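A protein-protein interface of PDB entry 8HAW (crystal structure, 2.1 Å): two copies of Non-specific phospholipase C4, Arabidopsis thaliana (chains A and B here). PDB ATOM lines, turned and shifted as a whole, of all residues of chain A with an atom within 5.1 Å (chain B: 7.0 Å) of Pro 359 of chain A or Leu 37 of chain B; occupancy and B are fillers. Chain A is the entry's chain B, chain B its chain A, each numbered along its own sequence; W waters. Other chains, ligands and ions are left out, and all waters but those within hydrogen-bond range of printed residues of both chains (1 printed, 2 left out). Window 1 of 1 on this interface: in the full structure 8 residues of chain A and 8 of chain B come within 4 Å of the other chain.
NZ of Lys 138 of chain B sits at hydrogen-bond distance from OD1 of Asn 132 of chain B (2.7 Å).
The side-chain amide oxygen (OD1) of Asn 38 of chain B lies close to the backbone NH (N) of Glu 40 of chain B, 3.2 Å away.
N of Tyr 360 of chain A lies within hydrogen-bond range of OG of Ser 363 of chain A (2.8 Å).
The backbone carbonyl oxygen (O) of Leu 37 of chain B is in hydrogen-bond range of the side-chain amide nitrogen (NE2) of Gln 142 of chain B.
The side-chain amino group (NZ) of Lys 35 of chain B sits at hydrogen-bond distance from the backbone carbonyl oxygen (O) of Arg 39 of chain B, at 2.9 Å.
Of the printed residues of chain B, Asn 357 of chain A touches Glu 36 (3.8 Å), Leu 37 (3.8 Å) and Lys 138 (3.0 Å).
Printed residues of chain B within 4 Å of Gly 358 of chain A: Glu 36 and Leu 37.
Of the printed residues of chain B, Ser 389 of chain A touches Arg 39.
Of chain A, only Asn 357 (3.8 Å), Gly 358 (3.9 Å), Pro 359 (3.5 Å), Tyr 360 (3.1 Å) and Pro 361 (3.2 Å) come within 4 Å of Leu 37 of chain B.
Water W1 lies within hydrogen-bond range of OH of Tyr 360 of chain A (2.7 Å) and OE2 of Glu 40 of chain B (2.8 Å).
O of Glu 36 of chain B touches O of Asn 357 of chain A, 3.8 Å away.
Asn 357 of chain A touches Leu 37 of chain B.
Glu 36 of chain B touches Gly 358 of chain A (O to CA, 3.3 Å).
Gly 358 of chain A touches Leu 37 of chain B.
O of Glu 36 of chain B touches CA of Pro 359 of chain A, at 3.5 Å.
O of Leu 37 of chain B touches O of Pro 359 of chain A, at 3.5 Å.
Pro 359 of chain A touches Asn 38 of chain B (O to CA, 3.3 Å).
Tyr 360 of chain A touches Leu 37 of chain B.
CD1 of Tyr 360 of chain A touches OD1 of Asn 38 of chain B, at 3.8 Å.
Pro 361 of chain A touches Gln 142 of chain B (CA to NE2, 3.3 Å).
No position is printed for both chains.
Of the 16 pairs that touch across the chains among the printed residues, none has its exchanged pair printed and touching as well.
NH1 of Arg 39 of chain B is in hydrogen-bond range of OG of Ser 389 of chain A (3.0 Å).
The backbone nitrogen (N) of Pro 361 of chain A sits close to the backbone carbonyl oxygen (O) of Leu 37 of chain B (3.2 Å).
The backbone NH (N) of Arg 39 of chain B lies within hydrogen-bond range of the backbone carbonyl oxygen (O) of Pro 359 of chain A, 3.0 Å away.
OD1 of Asn 357 of chain A sits at hydrogen-bond distance from NZ of Lys 138 of chain B, 3.0 Å away.
The guanidinium group (NH1) of Arg 39 of chain B lies within hydrogen-bond range of the side-chain hydroxyl (OH) of Tyr 360 of chain A (3.0 Å).
Of the 15 printed residues of chain B, 6 touch a printed residue of chain A.
Of the 10 printed residues of chain A, 6 touch a printed residue of chain B.
Among the printed residues, 16 pairs touch across the chains.
Among the printed residues, no Asp or Glu carboxylate lies within 4 Å of a Lys or Arg side-chain nitrogen of the other chain.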
ATOM      1  N   ASN A 357      -1.865  15.457 -19.932  1.00  0.00           N
ATOM      2  CA  ASN A 357      -2.441  16.742 -20.324  1.00  0.00           C
ATOM      3  C   ASN A 357      -3.266  17.217 -19.133  1.00  0.00           C
ATOM      4  O   ASN A 357      -4.453  16.903 -19.020  1.00  0.00           O
ATOM      5  CB  ASN A 357      -3.286  16.622 -21.593  1.00  0.00           C
ATOM      6  CG  ASN A 357      -2.444  16.537 -22.849  1.00  0.00           C
ATOM      7  OD1 ASN A 357      -1.751  17.488 -23.212  1.00  0.00           O
ATOM      8  ND2 ASN A 357      -2.498  15.393 -23.522  1.00  0.00           N
ATOM      9  N   GLY A 358      -2.627  17.959 -18.233  1.00  0.00           N
ATOM     10  CA  GLY A 358      -3.272  18.393 -17.018  1.00  0.00           C
ATOM     11  C   GLY A 358      -3.163  17.348 -15.925  1.00  0.00           C
ATOM     12  O   GLY A 358      -2.547  16.292 -16.107  1.00  0.00           O
ATOM     13  N   PRO A 359      -3.787  17.609 -14.766  1.00  0.00           N
ATOM     14  CA  PRO A 359      -4.629  18.776 -14.478  1.00  0.00           C
ATOM     15  C   PRO A 359      -3.866  20.076 -14.197  1.00  0.00           C
ATOM     16  O   PRO A 359      -4.502  21.113 -14.006  1.00  0.00           O
ATOM     17  CB  PRO A 359      -5.402  18.337 -13.233  1.00  0.00           C
ATOM     18  CG  PRO A 359      -4.468  17.402 -12.545  1.00  0.00           C
ATOM     19  CD  PRO A 359      -3.790  16.645 -13.651  1.00  0.00           C
ATOM     20  N   TYR A 360      -2.542  20.026 -14.178  1.00  0.00           N
ATOM     21  CA  TYR A 360      -1.708  21.195 -13.952  1.00  0.00           C
ATOM     22  C   TYR A 360      -0.588  21.235 -14.979  1.00  0.00           C
ATOM     23  O   TYR A 360      -0.240  20.207 -15.570  1.00  0.00           O
ATOM     24  CB  TYR A 360      -1.130  21.190 -12.529  1.00  0.00           C
ATOM     25  CG  TYR A 360      -2.183  21.383 -11.462  1.00  0.00           C
ATOM     26  CD1 TYR A 360      -2.772  22.624 -11.257  1.00  0.00           C
ATOM     27  CD2 TYR A 360      -2.593  20.323 -10.663  1.00  0.00           C
ATOM     28  CE1 TYR A 360      -3.738  22.806 -10.284  1.00  0.00           C
ATOM     29  CE2 TYR A 360      -3.556  20.494  -9.687  1.00  0.00           C
ATOM     30  CZ  TYR A 360      -4.125  21.737  -9.502  1.00  0.00           C
ATOM     31  OH  TYR A 360      -5.085  21.910  -8.532  1.00  0.00           O
ATOM     32  N   PRO A 361      -0.014  22.417 -15.231  1.00  0.00           N
ATOM     33  CA  PRO A 361       1.029  22.513 -16.268  1.00  0.00           C
ATOM     34  C   PRO A 361       2.238  21.631 -16.014  1.00  0.00           C
ATOM     35  O   PRO A 361       2.842  21.138 -16.975  1.00  0.00           O
ATOM     36  CB  PRO A 361       1.401  24.003 -16.241  1.00  0.00           C
ATOM     37  CG  PRO A 361       0.164  24.675 -15.745  1.00  0.00           C
ATOM     38  CD  PRO A 361      -0.368  23.744 -14.696  1.00  0.00           C
ATOM     39  N   SER A 363       2.084  18.790 -14.223  1.00  0.00           N
ATOM     40  CA  SER A 363       1.608  17.468 -13.842  1.00  0.00           C
ATOM     41  C   SER A 363       2.426  16.384 -14.533  1.00  0.00           C
ATOM     42  O   SER A 363       2.931  16.565 -15.645  1.00  0.00           O
ATOM     43  CB  SER A 363       0.128  17.311 -14.195  1.00  0.00           C
ATOM     44  OG  SER A 363      -0.688  18.101 -13.348  1.00  0.00           O
ATOM     45  N   SER A 389      -4.171  14.601  -6.433  1.00  0.00           N
ATOM     46  CA  SER A 389      -4.852  15.785  -6.943  1.00  0.00           C
ATOM     47  C   SER A 389      -4.067  16.423  -8.081  1.00  0.00           C
ATOM     48  O   SER A 389      -4.658  17.034  -8.979  1.00  0.00           O
ATOM     49  CB  SER A 389      -5.070  16.794  -5.814  1.00  0.00           C
ATOM     50  OG  SER A 389      -5.590  18.016  -6.310  1.00  0.00           O
ATOM     51  N   TRP A 390      -2.741  16.279  -8.066  1.00  0.00           N
ATOM     52  CA  TRP A 390      -1.871  16.887  -9.063  1.00  0.00           C
ATOM     53  C   TRP A 390      -1.432  15.923 -10.159  1.00  0.00           C
ATOM     54  O   TRP A 390      -1.111  16.372 -11.264  1.00  0.00           O
ATOM     55  CB  TRP A 390      -0.642  17.481  -8.357  1.00  0.00           C
ATOM     56  CG  TRP A 390       0.564  17.735  -9.209  1.00  0.00           C
ATOM     57  CD1 TRP A 390       0.898  18.903  -9.827  1.00  0.00           C
ATOM     58  CD2 TRP A 390       1.626  16.815  -9.491  1.00  0.00           C
ATOM     59  NE1 TRP A 390       2.088  18.763 -10.495  1.00  0.00           N
ATOM     60  CE2 TRP A 390       2.557  17.490 -10.305  1.00  0.00           C
ATOM     61  CE3 TRP A 390       1.874  15.482  -9.145  1.00  0.00           C
ATOM     62  CZ2 TRP A 390       3.717  16.880 -10.775  1.00  0.00           C
ATOM     63  CZ3 TRP A 390       3.026  14.879  -9.615  1.00  0.00           C
ATOM     64  CH2 TRP A 390       3.933  15.577 -10.421  1.00  0.00           C
ATOM     65  N   ALA A 391      -1.435  14.618  -9.893  1.00  0.00           N
ATOM     66  CA  ALA A 391      -0.901  13.653 -10.843  1.00  0.00           C
ATOM     67  C   ALA A 391      -1.788  13.538 -12.079  1.00  0.00           C
ATOM     68  O   ALA A 391      -3.002  13.750 -12.027  1.00  0.00           O
ATOM     69  CB  ALA A 391      -0.754  12.282 -10.185  1.00  0.00           C
ATOM     70  N   GLY A 392      -1.162  13.193 -13.201  1.00  0.00           N
ATOM     71  CA  GLY A 392      -1.918  12.941 -14.411  1.00  0.00           C
ATOM     72  C   GLY A 392      -2.772  11.694 -14.286  1.00  0.00           C
ATOM     73  O   GLY A 392      -2.471  10.777 -13.524  1.00  0.00           O
ATOM     74  N   TRP B  33     -11.429  25.958 -22.052  1.00  0.00           N
ATOM     75  CA  TRP B  33     -11.121  24.543 -21.940  1.00  0.00           C
ATOM     76  C   TRP B  33      -9.661  24.295 -21.589  1.00  0.00           C
ATOM     77  O   TRP B  33      -9.272  23.140 -21.399  1.00  0.00           O
ATOM     78  CB  TRP B  33     -11.505  23.835 -23.240  1.00  0.00           C
ATOM     79  CG  TRP B  33     -12.967  23.994 -23.529  1.00  0.00           C
ATOM     80  CD1 TRP B  33     -13.538  24.793 -24.477  1.00  0.00           C
ATOM     81  CD2 TRP B  33     -14.049  23.371 -22.826  1.00  0.00           C
ATOM     82  NE1 TRP B  33     -14.907  24.692 -24.420  1.00  0.00           N
ATOM     83  CE2 TRP B  33     -15.246  23.825 -23.415  1.00  0.00           C
ATOM     84  CE3 TRP B  33     -14.120  22.467 -21.760  1.00  0.00           C
ATOM     85  CZ2 TRP B  33     -16.501  23.404 -22.974  1.00  0.00           C
ATOM     86  CZ3 TRP B  33     -15.365  22.051 -21.326  1.00  0.00           C
ATOM     87  CH2 TRP B  33     -16.539  22.518 -21.932  1.00  0.00           C
ATOM     88  N   PHE B  34      -8.851  25.351 -21.481  1.00  0.00           N
ATOM     89  CA  PHE B  34      -7.508  25.207 -20.937  1.00  0.00           C
ATOM     90  C   PHE B  34      -7.524  24.903 -19.444  1.00  0.00           C
ATOM     91  O   PHE B  34      -6.471  24.579 -18.886  1.00  0.00           O
ATOM     92  CB  PHE B  34      -6.680  26.470 -21.198  1.00  0.00           C
ATOM     93  CG  PHE B  34      -6.216  26.617 -22.627  1.00  0.00           C
ATOM     94  CD1 PHE B  34      -7.098  26.468 -23.685  1.00  0.00           C
ATOM     95  CD2 PHE B  34      -4.892  26.910 -22.907  1.00  0.00           C
ATOM     96  CE1 PHE B  34      -6.670  26.608 -24.992  1.00  0.00           C
ATOM     97  CE2 PHE B  34      -4.458  27.050 -24.212  1.00  0.00           C
ATOM     98  CZ  PHE B  34      -5.349  26.898 -25.256  1.00  0.00           C
ATOM     99  N   LYS B  35      -8.687  25.002 -18.792  1.00  0.00           N
ATOM    100  CA  LYS B  35      -8.807  24.569 -17.405  1.00  0.00           C
ATOM    101  C   LYS B  35      -8.486  23.088 -17.246  1.00  0.00           C
ATOM    102  O   LYS B  35      -8.103  22.663 -16.150  1.00  0.00           O
ATOM    103  CB  LYS B  35     -10.214  24.870 -16.878  1.00  0.00           C
ATOM    104  CG  LYS B  35     -10.374  24.710 -15.368  1.00  0.00           C
ATOM    105  CD  LYS B  35     -11.772  25.102 -14.905  1.00  0.00           C
ATOM    106  CE  LYS B  35     -11.949  24.887 -13.407  1.00  0.00           C
ATOM    107  NZ  LYS B  35     -11.352  25.990 -12.595  1.00  0.00           N
ATOM    108  N   GLU B  36      -8.633  22.294 -18.314  1.00  0.00           N
ATOM    109  CA  GLU B  36      -8.169  20.911 -18.271  1.00  0.00           C
ATOM    110  C   GLU B  36      -6.667  20.837 -18.044  1.00  0.00           C
ATOM    111  O   GLU B  36      -6.178  19.886 -17.425  1.00  0.00           O
ATOM    112  CB  GLU B  36      -8.522  20.173 -19.566  1.00  0.00           C
ATOM    113  CG  GLU B  36      -9.963  20.289 -20.031  1.00  0.00           C
ATOM    114  CD  GLU B  36     -10.078  20.296 -21.546  1.00  0.00           C
ATOM    115  OE1 GLU B  36     -11.039  20.893 -22.074  1.00  0.00           O
ATOM    116  OE2 GLU B  36      -9.196  19.707 -22.209  1.00  0.00           O
ATOM    117  N   LEU B  37      -5.922  21.823 -18.543  1.00  0.00           N
ATOM    118  CA  LEU B  37      -4.471  21.828 -18.435  1.00  0.00           C
ATOM    119  C   LEU B  37      -3.969  22.594 -17.221  1.00  0.00           C
ATOM    120  O   LEU B  37      -2.811  22.415 -16.827  1.00  0.00           O
ATOM    121  CB  LEU B  37      -3.858  22.421 -19.707  1.00  0.00           C
ATOM    122  CG  LEU B  37      -4.403  21.838 -21.012  1.00  0.00           C
ATOM    123  CD1 LEU B  37      -3.861  22.598 -22.213  1.00  0.00           C
ATOM    124  CD2 LEU B  37      -4.075  20.353 -21.115  1.00  0.00           C
ATOM    125  N   ASN B  38      -4.806  23.441 -16.626  1.00  0.00           N
ATOM    126  CA  ASN B  38      -4.445  24.149 -15.400  1.00  0.00           C
ATOM    127  C   ASN B  38      -5.734  24.430 -14.641  1.00  0.00           C
ATOM    128  O   ASN B  38      -6.504  25.315 -15.028  1.00  0.00           O
ATOM    129  CB  ASN B  38      -3.683  25.437 -15.702  1.00  0.00           C
ATOM    130  CG  ASN B  38      -3.119  26.092 -14.449  1.00  0.00           C
ATOM    131  OD1 ASN B  38      -3.449  25.708 -13.327  1.00  0.00           O
ATOM    132  ND2 ASN B  38      -2.255  27.082 -14.641  1.00  0.00           N
ATOM    133  N   ARG B  39      -5.957  23.677 -13.561  1.00  0.00           N
ATOM    134  CA  ARG B  39      -7.187  23.788 -12.786  1.00  0.00           C
ATOM    135  C   ARG B  39      -7.384  25.179 -12.197  1.00  0.00           C
ATOM    136  O   ARG B  39      -8.523  25.562 -11.908  1.00  0.00           O
ATOM    137  CB  ARG B  39      -7.180  22.736 -11.674  1.00  0.00           C
ATOM    138  CG  ARG B  39      -8.529  22.456 -11.036  1.00  0.00           C
ATOM    139  CD  ARG B  39      -8.379  21.409  -9.942  1.00  0.00           C
ATOM    140  NE  ARG B  39      -8.111  20.087 -10.496  1.00  0.00           N
ATOM    141  CZ  ARG B  39      -7.370  19.161  -9.903  1.00  0.00           C
ATOM    142  NH1 ARG B  39      -6.782  19.386  -8.739  1.00  0.00           N
ATOM    143  NH2 ARG B  39      -7.212  17.980 -10.494  1.00  0.00           N
ATOM    144  N   GLU B  40      -6.305  25.946 -12.018  1.00  0.00           N
ATOM    145  CA  GLU B  40      -6.408  27.293 -11.471  1.00  0.00           C
ATOM    146  C   GLU B  40      -7.023  28.287 -12.448  1.00  0.00           C
ATOM    147  O   GLU B  40      -7.401  29.387 -12.027  1.00  0.00           O
ATOM    148  CB  GLU B  40      -5.028  27.790 -11.039  1.00  0.00           C
ATOM    149  CG  GLU B  40      -4.626  27.377  -9.633  1.00  0.00           C
ATOM    150  CD  GLU B  40      -5.589  27.886  -8.578  1.00  0.00           C
ATOM    151  OE1 GLU B  40      -5.713  29.120  -8.431  1.00  0.00           O
ATOM    152  OE2 GLU B  40      -6.221  27.053  -7.894  1.00  0.00           O
ATOM    153  N   ILE B  41      -7.129  27.940 -13.731  1.00  0.00           N
ATOM    154  CA  ILE B  41      -7.712  28.850 -14.709  1.00  0.00           C
ATOM    155  C   ILE B  41      -9.219  28.915 -14.509  1.00  0.00           C
ATOM    156  O   ILE B  41      -9.903  27.883 -14.478  1.00  0.00           O
ATOM    157  CB  ILE B  41      -7.367  28.403 -16.138  1.00  0.00           C
ATOM    158  CG1 ILE B  41      -5.867  28.533 -16.400  1.00  0.00           C
ATOM    159  CG2 ILE B  41      -8.164  29.214 -17.157  1.00  0.00           C
ATOM    160  CD1 ILE B  41      -5.428  27.931 -17.720  1.00  0.00           C
ATOM    161  N   PRO B 131      -7.990  22.796 -26.542  1.00  0.00           N
ATOM    162  CA  PRO B 131      -6.619  23.329 -26.460  1.00  0.00           C
ATOM    163  C   PRO B 131      -5.723  22.885 -27.605  1.00  0.00           C
ATOM    164  O   PRO B 131      -4.937  23.693 -28.116  1.00  0.00           O
ATOM    165  CB  PRO B 131      -6.131  22.796 -25.106  1.00  0.00           C
ATOM    166  CG  PRO B 131      -7.379  22.674 -24.294  1.00  0.00           C
ATOM    167  CD  PRO B 131      -8.434  22.210 -25.265  1.00  0.00           C
ATOM    168  N   ASN B 132      -5.841  21.629 -28.042  1.00  0.00           N
ATOM    169  CA  ASN B 132      -5.010  21.137 -29.136  1.00  0.00           C
ATOM    170  C   ASN B 132      -5.299  21.848 -30.451  1.00  0.00           C
ATOM    171  O   ASN B 132      -4.441  21.854 -31.341  1.00  0.00           O
ATOM    172  CB  ASN B 132      -5.200  19.628 -29.303  1.00  0.00           C
ATOM    173  CG  ASN B 132      -4.352  18.826 -28.336  1.00  0.00           C
ATOM    174  OD1 ASN B 132      -3.501  19.375 -27.636  1.00  0.00           O
ATOM    175  ND2 ASN B 132      -4.577  17.517 -28.294  1.00  0.00           N
ATOM    176  N   LYS B 138      -1.536  26.811 -26.517  1.00  0.00           N
ATOM    177  CA  LYS B 138      -1.333  25.761 -25.523  1.00  0.00           C
ATOM    178  C   LYS B 138       0.069  25.836 -24.929  1.00  0.00           C
ATOM    179  O   LYS B 138       0.239  25.906 -23.703  1.00  0.00           O
ATOM    180  CB  LYS B 138      -1.581  24.387 -26.149  1.00  0.00           C
ATOM    181  CG  LYS B 138      -1.525  23.237 -25.155  1.00  0.00           C
ATOM    182  CD  LYS B 138      -1.842  21.902 -25.813  1.00  0.00           C
ATOM    183  CE  LYS B 138      -1.730  20.758 -24.815  1.00  0.00           C
ATOM    184  NZ  LYS B 138      -1.851  19.424 -25.472  1.00  0.00           N
ATOM    185  N   GLU B 139       1.089  25.851 -25.793  1.00  0.00           N
ATOM    186  CA  GLU B 139       2.463  25.889 -25.302  1.00  0.00           C
ATOM    187  C   GLU B 139       2.756  27.184 -24.555  1.00  0.00           C
ATOM    188  O   GLU B 139       3.410  27.167 -23.504  1.00  0.00           O
ATOM    189  CB  GLU B 139       3.444  25.705 -26.459  1.00  0.00           C
ATOM    190  CG  GLU B 139       4.704  24.952 -26.068  1.00  0.00           C
ATOM    191  CD  GLU B 139       5.634  24.718 -27.240  1.00  0.00           C
ATOM    192  OE1 GLU B 139       5.148  24.682 -28.391  1.00  0.00           O
ATOM    193  OE2 GLU B 139       6.852  24.565 -27.010  1.00  0.00           O
ATOM    194  N   VAL B 141       0.659  29.227 -22.944  1.00  0.00           N
ATOM    195  CA  VAL B 141      -0.032  29.241 -21.660  1.00  0.00           C
ATOM    196  C   VAL B 141       0.667  28.319 -20.672  1.00  0.00           C
ATOM    197  O   VAL B 141       0.837  28.665 -19.497  1.00  0.00           O
ATOM    198  CB  VAL B 141      -1.512  28.855 -21.843  1.00  0.00           C
ATOM    199  CG1 VAL B 141      -2.157  28.549 -20.499  1.00  0.00           C
ATOM    200  CG2 VAL B 141      -2.268  29.962 -22.557  1.00  0.00           C
ATOM    201  N   GLN B 142       1.094  27.140 -21.130  1.00  0.00           N
ATOM    202  CA  GLN B 142       1.752  26.221 -20.211  1.00  0.00           C
ATOM    203  C   GLN B 142       3.151  26.684 -19.820  1.00  0.00           C
ATOM    204  O   GLN B 142       3.650  26.275 -18.766  1.00  0.00           O
ATOM    205  CB  GLN B 142       1.806  24.821 -20.823  1.00  0.00           C
ATOM    206  CG  GLN B 142       0.465  24.062 -20.903  1.00  0.00           C
ATOM    207  CD  GLN B 142      -0.419  24.165 -19.655  1.00  0.00           C
ATOM    208  OE1 GLN B 142      -0.849  25.249 -19.249  1.00  0.00           O
ATOM    209  NE2 GLN B 142      -0.690  23.020 -19.044  1.00  0.00           N
HETATM  210  O   HOH W   1      -6.274  24.301  -8.157  1.00  0.00           O
